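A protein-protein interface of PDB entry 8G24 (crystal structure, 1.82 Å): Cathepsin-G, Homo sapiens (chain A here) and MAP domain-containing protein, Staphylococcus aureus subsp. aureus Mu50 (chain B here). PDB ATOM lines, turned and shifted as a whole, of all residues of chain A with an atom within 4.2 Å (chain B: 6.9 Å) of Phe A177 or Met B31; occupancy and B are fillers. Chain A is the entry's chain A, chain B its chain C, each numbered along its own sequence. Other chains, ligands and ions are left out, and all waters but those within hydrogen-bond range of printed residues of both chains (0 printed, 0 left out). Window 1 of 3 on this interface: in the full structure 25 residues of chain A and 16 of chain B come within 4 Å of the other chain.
NZ of Lys A199 sits at hydrogen-bond distance from O of Gly B29 (2.6 Å). N of Met B31 lies within hydrogen-bond range of O of Gly A198 (2.8 Å). The backbone carbonyl oxygen (O) of Phe B33 is in hydrogen-bond range of the backbone NH (N) of Gly A179 (2.7 Å). The backbone NH of Asp A180 lies within hydrogen-bond range of the backbone carbonyl oxygen of Phe B33. O of Phe A177 lies close to O of Phe B33, at 3.4 Å.
OG1 of Thr B24 is in hydrogen-bond range of OD1 of Asp B111 (2.7 Å). NH1 of Arg B63 lies within hydrogen-bond range of O of Ile B30 (3.0 Å). The backbone carbonyl oxygen (O) of Lys A178 sits at hydrogen-bond distance from the backbone NH (N) of Arg A129, at 2.8 Å. The side-chain carboxylate (OD2) of Asp A180 sits at hydrogen-bond distance from the backbone NH (N) of Phe A177 (2.8 Å).
Among the printed residues, merely in contact across the chains: Arg A129 with Gln B35 (2.9 Å), Tyr A197 with Met B31 (3.2 Å), Ala A176 with Phe B33 (3.4 Å), Gly A179 with Asn B34 (3.4 Å), Gly A198 with Phe B33 (3.6 Å), Gly A179 with Gln B35 (3.6 Å), Lys A178 with Phe B33 (3.6 Å), Ser A200 with Met B31 (3.6 Å), Lys A178 with Thr B24 (3.6 Å), Lys A199 with Phe B33 (3.7 Å), Tyr A197 with Ile B30 (3.7 Å), Lys A178 with Asn B34 (3.7 Å), Gly A198 with Ile B30 (3.7 Å), Lys A199 with Met B31 (3.8 Å), Lys A178 with Met B31 (3.8 Å), Tyr A197 with Phe B33 (3.8 Å), Lys A178 with Gln B35 (3.9 Å), Phe A177 with Met B31 (3.9 Å), Tyr A197 with Ala B32 (3.9 Å) and Gly A198 with Gly B29 (3.9 Å).
Phe A177 touches just these residues of chain B: Met B31 (3.9 Å) and Phe B33 (3.4 Å). Of chain A, only Phe A177, Lys A178, Tyr A197, Gly A198, Lys A199 and Ser A200 come within 4 Å of Met B31. Of the printed residues of chain A, Asn B34 touches Lys A178 (3.7 Å) and Gly A179 (3.4 Å). Of the printed residues of chain B, Ala A176 touches Phe B33 (3.4 Å). Of the printed residues of chain B, Gly A198 touches Gly B29 (3.9 Å), Ile B30 (3.7 Å), Met B31 (2.8 Å) and Phe B33 (3.6 Å). Printed residues of chain B within 4 Å of Gly A179: Phe B33, Asn B34 and Gln B35. Printed residues of chain A within 4 Å of Thr B24: Lys A178. Ser A201 touches none of the printed residues of chain B. The nearest residue of chain B that does not touch Phe A177 is Asn B34 (5.5 Å). The nearest printed residue of chain B that does not touch Asp A180 is Asn B34 (5.3 Å).
Printed residues of chain B that touch a printed residue of chain A: Thr B24, Gly B29, Ile B30, Met B31, Ala B32, Phe B33, Asn B34 and Gln B35. Along chain B the printed residues that touch a printed residue of chain A span positions 24 to 35. Printed residues of chain A that touch a printed residue of chain B: Arg A129, Ala A176, Phe A177, Lys A178, Gly A179, Asp A180, Tyr A197, Gly A198, Lys A199 and Ser A200. Hydrophobic or aromatic side chains of chain A that line the printed part of chain B: Phe A177 and Tyr A197. Among the printed residues, no Asp or Glu carboxylate lies within 4 Å of a Lys or Arg side-chain nitrogen of the other chain.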
ATOM      1  N   ILE A   2       0.442 -29.309 -24.340  1.00  0.00           N
ATOM      2  CA  ILE A   2       1.314 -29.227 -23.173  1.00  0.00           C
ATOM      3  C   ILE A   2       1.845 -30.617 -22.856  1.00  0.00           C
ATOM      4  O   ILE A   2       1.077 -31.585 -22.812  1.00  0.00           O
ATOM      5  CB  ILE A   2       0.560 -28.677 -21.953  1.00  0.00           C
ATOM      6  CG1 ILE A   2       0.114 -27.245 -22.153  1.00  0.00           C
ATOM      7  CG2 ILE A   2       1.466 -28.774 -20.705  1.00  0.00           C
ATOM      8  CD1 ILE A   2      -0.943 -26.824 -21.142  1.00  0.00           C
ATOM      9  N   ARG A 129      -0.369 -23.745 -28.176  1.00  0.00           N
ATOM     10  CA  ARG A 129       0.679 -23.344 -27.243  1.00  0.00           C
ATOM     11  C   ARG A 129       1.121 -24.519 -26.373  1.00  0.00           C
ATOM     12  O   ARG A 129       0.348 -25.422 -26.069  1.00  0.00           O
ATOM     13  CB  ARG A 129       0.193 -22.216 -26.331  1.00  0.00           C
ATOM     14  CG  ARG A 129      -0.447 -21.028 -27.037  1.00  0.00           C
ATOM     15  CD  ARG A 129       0.578 -20.057 -27.620  1.00  0.00           C
ATOM     16  NE  ARG A 129       1.448 -19.420 -26.628  1.00  0.00           N
ATOM     17  CZ  ARG A 129       2.432 -18.579 -26.931  1.00  0.00           C
ATOM     18  NH1 ARG A 129       2.707 -18.261 -28.184  1.00  0.00           N
ATOM     19  NH2 ARG A 129       3.156 -18.036 -25.954  1.00  0.00           N
ATOM     20  N   MET A 132       2.210 -21.230 -20.946  1.00  0.00           N
ATOM     21  CA  MET A 132       1.721 -19.863 -20.972  1.00  0.00           C
ATOM     22  C   MET A 132       2.623 -18.993 -21.836  1.00  0.00           C
ATOM     23  O   MET A 132       2.145 -18.101 -22.542  1.00  0.00           O
ATOM     24  CB  MET A 132       1.634 -19.311 -19.551  1.00  0.00           C
ATOM     25  CG  MET A 132       0.792 -20.153 -18.585  1.00  0.00           C
ATOM     26  SD  MET A 132      -0.919 -20.437 -19.082  1.00  0.00           S
ATOM     27  CE  MET A 132      -1.304 -18.913 -19.937  1.00  0.00           C
ATOM     28  N   ALA A 175      -1.750 -32.211 -21.818  1.00  0.00           N
ATOM     29  CA  ALA A 175      -3.094 -31.775 -22.188  1.00  0.00           C
ATOM     30  C   ALA A 175      -3.067 -31.089 -23.551  1.00  0.00           C
ATOM     31  O   ALA A 175      -2.002 -30.747 -24.068  1.00  0.00           O
ATOM     32  CB  ALA A 175      -3.687 -30.823 -21.137  1.00  0.00           C
ATOM     33  N   ALA A 176      -4.253 -30.931 -24.144  1.00  0.00           N
ATOM     34  CA  ALA A 176      -4.432 -29.966 -25.220  1.00  0.00           C
ATOM     35  C   ALA A 176      -4.565 -28.569 -24.622  1.00  0.00           C
ATOM     36  O   ALA A 176      -4.894 -28.411 -23.439  1.00  0.00           O
ATOM     37  CB  ALA A 176      -5.658 -30.301 -26.056  1.00  0.00           C
ATOM     38  N   PHE A 177      -4.226 -27.556 -25.412  1.00  0.00           N
ATOM     39  CA  PHE A 177      -4.256 -26.189 -24.882  1.00  0.00           C
ATOM     40  C   PHE A 177      -4.565 -25.215 -26.017  1.00  0.00           C
ATOM     41  O   PHE A 177      -5.091 -25.615 -27.057  1.00  0.00           O
ATOM     42  CB  PHE A 177      -2.954 -25.921 -24.130  1.00  0.00           C
ATOM     43  CG  PHE A 177      -3.031 -24.776 -23.128  1.00  0.00           C
ATOM     44  CD1 PHE A 177      -4.084 -24.653 -22.233  1.00  0.00           C
ATOM     45  CD2 PHE A 177      -2.043 -23.816 -23.107  1.00  0.00           C
ATOM     46  CE1 PHE A 177      -4.135 -23.601 -21.348  1.00  0.00           C
ATOM     47  CE2 PHE A 177      -2.083 -22.762 -22.221  1.00  0.00           C
ATOM     48  CZ  PHE A 177      -3.136 -22.654 -21.335  1.00  0.00           C
ATOM     49  N   LYS A 178      -4.264 -23.931 -25.807  1.00  0.00           N
ATOM     50  CA  LYS A 178      -4.797 -22.880 -26.665  1.00  0.00           C
ATOM     51  C   LYS A 178      -4.253 -23.024 -28.078  1.00  0.00           C
ATOM     52  O   LYS A 178      -3.039 -23.030 -28.291  1.00  0.00           O
ATOM     53  CB  LYS A 178      -4.427 -21.507 -26.090  1.00  0.00           C
ATOM     54  CG  LYS A 178      -5.122 -21.167 -24.767  1.00  0.00           C
ATOM     55  CD  LYS A 178      -4.814 -19.742 -24.273  1.00  0.00           C
ATOM     56  CE  LYS A 178      -3.443 -19.656 -23.620  1.00  0.00           C
ATOM     57  NZ  LYS A 178      -3.294 -18.455 -22.750  1.00  0.00           N
ATOM     58  N   GLY A 179      -5.156 -23.080 -29.040  1.00  0.00           N
ATOM     59  CA  GLY A 179      -4.831 -23.285 -30.434  1.00  0.00           C
ATOM     60  C   GLY A 179      -5.035 -24.712 -30.907  1.00  0.00           C
ATOM     61  O   GLY A 179      -4.964 -24.971 -32.110  1.00  0.00           O
ATOM     62  N   ASP A 180      -5.220 -25.646 -29.987  1.00  0.00           N
ATOM     63  CA  ASP A 180      -5.522 -27.041 -30.321  1.00  0.00           C
ATOM     64  C   ASP A 180      -7.001 -27.337 -30.559  1.00  0.00           C
ATOM     65  O   ASP A 180      -7.325 -28.424 -31.082  1.00  0.00           O
ATOM     66  CB  ASP A 180      -4.995 -27.940 -29.186  1.00  0.00           C
ATOM     67  CG  ASP A 180      -3.517 -27.914 -29.062  1.00  0.00           C
ATOM     68  OD1 ASP A 180      -2.862 -27.862 -30.121  1.00  0.00           O
ATOM     69  OD2 ASP A 180      -2.974 -27.895 -27.912  1.00  0.00           O
ATOM     70  N   TYR A 197     -12.713 -27.636 -24.885  1.00  0.00           N
ATOM     71  CA  TYR A 197     -12.442 -26.649 -23.847  1.00  0.00           C
ATOM     72  C   TYR A 197     -11.827 -27.294 -22.611  1.00  0.00           C
ATOM     73  O   TYR A 197     -11.771 -28.515 -22.469  1.00  0.00           O
ATOM     74  CB  TYR A 197     -13.683 -25.843 -23.424  1.00  0.00           C
ATOM     75  CG  TYR A 197     -14.794 -26.615 -22.696  1.00  0.00           C
ATOM     76  CD1 TYR A 197     -14.673 -26.963 -21.350  1.00  0.00           C
ATOM     77  CD2 TYR A 197     -15.976 -26.952 -23.343  1.00  0.00           C
ATOM     78  CE1 TYR A 197     -15.672 -27.645 -20.692  1.00  0.00           C
ATOM     79  CE2 TYR A 197     -16.987 -27.623 -22.692  1.00  0.00           C
ATOM     80  CZ  TYR A 197     -16.851 -27.965 -21.366  1.00  0.00           C
ATOM     81  OH  TYR A 197     -17.883 -28.600 -20.710  1.00  0.00           O
ATOM     82  N   GLY A 198     -11.344 -26.421 -21.722  1.00  0.00           N
ATOM     83  CA  GLY A 198     -10.869 -26.831 -20.417  1.00  0.00           C
ATOM     84  C   GLY A 198     -10.639 -25.631 -19.521  1.00  0.00           C
ATOM     85  O   GLY A 198     -11.313 -24.614 -19.642  1.00  0.00           O
ATOM     86  N   LYS A 199      -9.677 -25.739 -18.616  1.00  0.00           N
ATOM     87  CA  LYS A 199      -9.342 -24.686 -17.678  1.00  0.00           C
ATOM     88  C   LYS A 199      -8.324 -23.730 -18.262  1.00  0.00           C
ATOM     89  O   LYS A 199      -7.462 -24.115 -19.055  1.00  0.00           O
ATOM     90  CB  LYS A 199      -8.767 -25.290 -16.392  1.00  0.00           C
ATOM     91  CG  LYS A 199      -9.764 -26.070 -15.563  1.00  0.00           C
ATOM     92  CD  LYS A 199     -10.600 -25.105 -14.756  1.00  0.00           C
ATOM     93  CE  LYS A 199     -11.858 -25.772 -14.277  1.00  0.00           C
ATOM     94  NZ  LYS A 199     -12.930 -24.769 -14.103  1.00  0.00           N
ATOM     95  N   SER A 200      -8.426 -22.466 -17.837  1.00  0.00           N
ATOM     96  CA  SER A 200      -7.463 -21.458 -18.263  1.00  0.00           C
ATOM     97  C   SER A 200      -6.035 -21.891 -17.956  1.00  0.00           C
ATOM     98  O   SER A 200      -5.095 -21.538 -18.685  1.00  0.00           O
ATOM     99  CB  SER A 200      -7.743 -20.128 -17.570  1.00  0.00           C
ATOM    100  OG  SER A 200      -7.593 -20.263 -16.182  1.00  0.00           O
ATOM    101  N   SER A 201      -5.858 -22.610 -16.850  1.00  0.00           N
ATOM    102  CA  SER A 201      -4.544 -23.098 -16.443  1.00  0.00           C
ATOM    103  C   SER A 201      -3.989 -24.162 -17.379  1.00  0.00           C
ATOM    104  O   SER A 201      -2.779 -24.398 -17.391  1.00  0.00           O
ATOM    105  CB  SER A 201      -4.629 -23.707 -15.050  1.00  0.00           C
ATOM    106  OG  SER A 201      -5.265 -24.987 -15.128  1.00  0.00           O
ATOM    107  N   GLY A 202      -4.839 -24.806 -18.156  1.00  0.00           N
ATOM    108  CA  GLY A 202      -4.458 -25.989 -18.893  1.00  0.00           C
ATOM    109  C   GLY A 202      -4.314 -27.264 -18.083  1.00  0.00           C
ATOM    110  O   GLY A 202      -3.886 -28.283 -18.630  1.00  0.00           O
ATOM    111  N   THR B  24      -7.825 -14.082 -23.921  1.00  0.00           N
ATOM    112  CA  THR B  24      -8.480 -15.316 -23.484  1.00  0.00           C
ATOM    113  C   THR B  24      -9.778 -14.971 -22.779  1.00  0.00           C
ATOM    114  O   THR B  24      -9.869 -13.947 -22.114  1.00  0.00           O
ATOM    115  CB  THR B  24      -7.641 -16.145 -22.501  1.00  0.00           C
ATOM    116  OG1 THR B  24      -7.517 -15.410 -21.281  1.00  0.00           O
ATOM    117  CG2 THR B  24      -6.264 -16.427 -23.074  1.00  0.00           C
ATOM    118  N   ILE B  25     -10.776 -15.844 -22.895  1.00  0.00           N
ATOM    119  CA  ILE B  25     -12.029 -15.693 -22.162  1.00  0.00           C
ATOM    120  C   ILE B  25     -12.281 -16.963 -21.359  1.00  0.00           C
ATOM    121  O   ILE B  25     -12.320 -18.064 -21.915  1.00  0.00           O
ATOM    122  CB  ILE B  25     -13.238 -15.422 -23.079  1.00  0.00           C
ATOM    123  CG1 ILE B  25     -13.072 -14.115 -23.845  1.00  0.00           C
ATOM    124  CG2 ILE B  25     -14.533 -15.395 -22.281  1.00  0.00           C
ATOM    125  CD1 ILE B  25     -14.121 -13.917 -24.914  1.00  0.00           C
ATOM    126  N   ALA B  26     -12.486 -16.806 -20.060  1.00  0.00           N
ATOM    127  CA  ALA B  26     -12.965 -17.872 -19.194  1.00  0.00           C
ATOM    128  C   ALA B  26     -14.283 -17.429 -18.574  1.00  0.00           C
ATOM    129  O   ALA B  26     -14.374 -16.327 -18.011  1.00  0.00           O
ATOM    130  CB  ALA B  26     -11.933 -18.215 -18.105  1.00  0.00           C
ATOM    131  N   VAL B  27     -15.311 -18.265 -18.710  1.00  0.00           N
ATOM    132  CA  VAL B  27     -16.609 -18.019 -18.091  1.00  0.00           C
ATOM    133  C   VAL B  27     -16.978 -19.260 -17.288  1.00  0.00           C
ATOM    134  O   VAL B  27     -17.031 -20.372 -17.830  1.00  0.00           O
ATOM    135  CB  VAL B  27     -17.710 -17.689 -19.123  1.00  0.00           C
ATOM    136  CG1 VAL B  27     -19.045 -17.491 -18.393  1.00  0.00           C
ATOM    137  CG2 VAL B  27     -17.356 -16.501 -19.958  1.00  0.00           C
ATOM    138  N   ASP B  28     -17.254 -19.066 -16.002  1.00  0.00           N
ATOM    139  CA  ASP B  28     -17.656 -20.170 -15.133  1.00  0.00           C
ATOM    140  C   ASP B  28     -16.660 -21.323 -15.228  1.00  0.00           C
ATOM    141  O   ASP B  28     -17.038 -22.497 -15.322  1.00  0.00           O
ATOM    142  CB  ASP B  28     -19.069 -20.644 -15.474  1.00  0.00           C
ATOM    143  CG  ASP B  28     -20.130 -19.667 -15.031  1.00  0.00           C
ATOM    144  OD1 ASP B  28     -20.013 -19.121 -13.913  1.00  0.00           O
ATOM    145  OD2 ASP B  28     -21.086 -19.430 -15.798  1.00  0.00           O
ATOM    146  N   GLY B  29     -15.370 -20.978 -15.258  1.00  0.00           N
ATOM    147  CA  GLY B  29     -14.356 -22.006 -15.223  1.00  0.00           C
ATOM    148  C   GLY B  29     -14.178 -22.777 -16.511  1.00  0.00           C
ATOM    149  O   GLY B  29     -13.556 -23.831 -16.492  1.00  0.00           O
ATOM    150  N   ILE B  30     -14.737 -22.304 -17.617  1.00  0.00           N
ATOM    151  CA  ILE B  30     -14.623 -22.941 -18.919  1.00  0.00           C
ATOM    152  C   ILE B  30     -13.930 -21.962 -19.867  1.00  0.00           C
ATOM    153  O   ILE B  30     -14.359 -20.803 -20.004  1.00  0.00           O
ATOM    154  CB  ILE B  30     -16.008 -23.322 -19.472  1.00  0.00           C
ATOM    155  CG1 ILE B  30     -16.569 -24.578 -18.857  1.00  0.00           C
ATOM    156  CG2 ILE B  30     -15.923 -23.469 -20.999  1.00  0.00           C
ATOM    157  CD1 ILE B  30     -18.067 -24.727 -19.100  1.00  0.00           C
ATOM    158  N   MET B  31     -12.857 -22.421 -20.516  1.00  0.00           N
ATOM    159  CA  MET B  31     -12.169 -21.641 -21.537  1.00  0.00           C
ATOM    160  C   MET B  31     -12.058 -22.477 -22.804  1.00  0.00           C
ATOM    161  O   MET B  31     -11.519 -23.582 -22.761  1.00  0.00           O
ATOM    162  CB  MET B  31     -10.775 -21.206 -21.056  1.00  0.00           C
ATOM    163  CG  MET B  31      -9.979 -20.379 -22.080  1.00  0.00           C
ATOM    164  SD  MET B  31      -8.275 -19.997 -21.442  1.00  0.00           S
ATOM    165  CE  MET B  31      -7.487 -21.585 -21.850  1.00  0.00           C
ATOM    166  N   ALA B  32     -12.569 -21.953 -23.918  1.00  0.00           N
ATOM    167  CA  ALA B  32     -12.368 -22.585 -25.216  1.00  0.00           C
ATOM    168  C   ALA B  32     -10.891 -22.590 -25.567  1.00  0.00           C
ATOM    169  O   ALA B  32     -10.149 -21.694 -25.190  1.00  0.00           O
ATOM    170  CB  ALA B  32     -13.146 -21.837 -26.282  1.00  0.00           C
ATOM    171  N   PHE B  33     -10.453 -23.629 -26.262  1.00  0.00           N
ATOM    172  CA  PHE B  33      -9.037 -23.821 -26.543  1.00  0.00           C
ATOM    173  C   PHE B  33      -8.631 -23.375 -27.959  1.00  0.00           C
ATOM    174  O   PHE B  33      -7.692 -23.931 -28.560  1.00  0.00           O
ATOM    175  CB  PHE B  33      -8.675 -25.282 -26.311  1.00  0.00           C
ATOM    176  CG  PHE B  33      -8.382 -25.634 -24.858  1.00  0.00           C
ATOM    177  CD1 PHE B  33      -8.139 -24.650 -23.901  1.00  0.00           C
ATOM    178  CD2 PHE B  33      -8.326 -26.963 -24.463  1.00  0.00           C
ATOM    179  CE1 PHE B  33      -7.869 -25.002 -22.597  1.00  0.00           C
ATOM    180  CE2 PHE B  33      -8.056 -27.314 -23.157  1.00  0.00           C
ATOM    181  CZ  PHE B  33      -7.822 -26.329 -22.221  1.00  0.00           C
ATOM    182  N   ASN B  34      -9.298 -22.371 -28.502  1.00  0.00           N
ATOM    183  CA  ASN B  34      -8.725 -21.686 -29.654  1.00  0.00           C
ATOM    184  C   ASN B  34      -7.646 -20.714 -29.180  1.00  0.00           C
ATOM    185  O   ASN B  34      -7.433 -20.502 -27.981  1.00  0.00           O
ATOM    186  CB  ASN B  34      -9.814 -20.987 -30.477  1.00  0.00           C
ATOM    187  CG  ASN B  34     -10.586 -19.948 -29.687  1.00  0.00           C
ATOM    188  OD1 ASN B  34     -10.609 -19.980 -28.458  1.00  0.00           O
ATOM    189  ND2 ASN B  34     -11.223 -19.020 -30.394  1.00  0.00           N
ATOM    190  N   GLN B  35      -6.903 -20.170 -30.141  1.00  0.00           N
ATOM    191  CA  GLN B  35      -5.913 -19.134 -29.878  1.00  0.00           C
ATOM    192  C   GLN B  35      -6.397 -17.889 -30.609  1.00  0.00           C
ATOM    193  O   GLN B  35      -6.380 -17.853 -31.835  1.00  0.00           O
ATOM    194  CB  GLN B  35      -4.522 -19.576 -30.334  1.00  0.00           C
ATOM    195  CG  GLN B  35      -3.459 -18.518 -30.178  1.00  0.00           C
ATOM    196  CD  GLN B  35      -2.066 -19.110 -30.043  1.00  0.00           C
ATOM    197  OE1 GLN B  35      -1.211 -18.539 -29.374  1.00  0.00           O
ATOM    198  NE2 GLN B  35      -1.828 -20.250 -30.698  1.00  0.00           N
ATOM    199  N   ARG B  63     -18.928 -15.772 -26.293  1.00  0.00           N
ATOM    200  CA  ARG B  63     -19.455 -16.650 -25.252  1.00  0.00           C
ATOM    201  C   ARG B  63     -20.874 -16.299 -24.811  1.00  0.00           C
ATOM    202  O   ARG B  63     -21.342 -16.837 -23.798  1.00  0.00           O
ATOM    203  CB  ARG B  63     -18.538 -16.631 -24.028  1.00  0.00           C
ATOM    204  CG  ARG B  63     -17.187 -17.371 -24.209  1.00  0.00           C
ATOM    205  CD  ARG B  63     -17.335 -18.830 -24.618  1.00  0.00           C
ATOM    206  NE  ARG B  63     -17.957 -19.652 -23.577  1.00  0.00           N
ATOM    207  CZ  ARG B  63     -17.361 -20.039 -22.454  1.00  0.00           C
ATOM    208  NH1 ARG B  63     -16.106 -19.694 -22.190  1.00  0.00           N
ATOM    209  NH2 ARG B  63     -18.043 -20.795 -21.580  1.00  0.00           N
ATOM    210  N   ASP B 111      -6.824 -10.828 -20.624  1.00  0.00           N
ATOM    211  CA  ASP B 111      -7.392 -12.058 -20.087  1.00  0.00           C
ATOM    212  C   ASP B 111      -8.680 -11.710 -19.361  1.00  0.00           C
ATOM    213  O   ASP B 111      -8.676 -10.923 -18.413  1.00  0.00           O
ATOM    214  CB  ASP B 111      -6.352 -12.739 -19.204  1.00  0.00           C
ATOM    215  CG  ASP B 111      -5.125 -13.185 -20.013  1.00  0.00           C
ATOM    216  OD1 ASP B 111      -5.302 -13.967 -20.981  1.00  0.00           O
ATOM    217  OD2 ASP B 111      -3.999 -12.738 -19.706  1.00  0.00           O
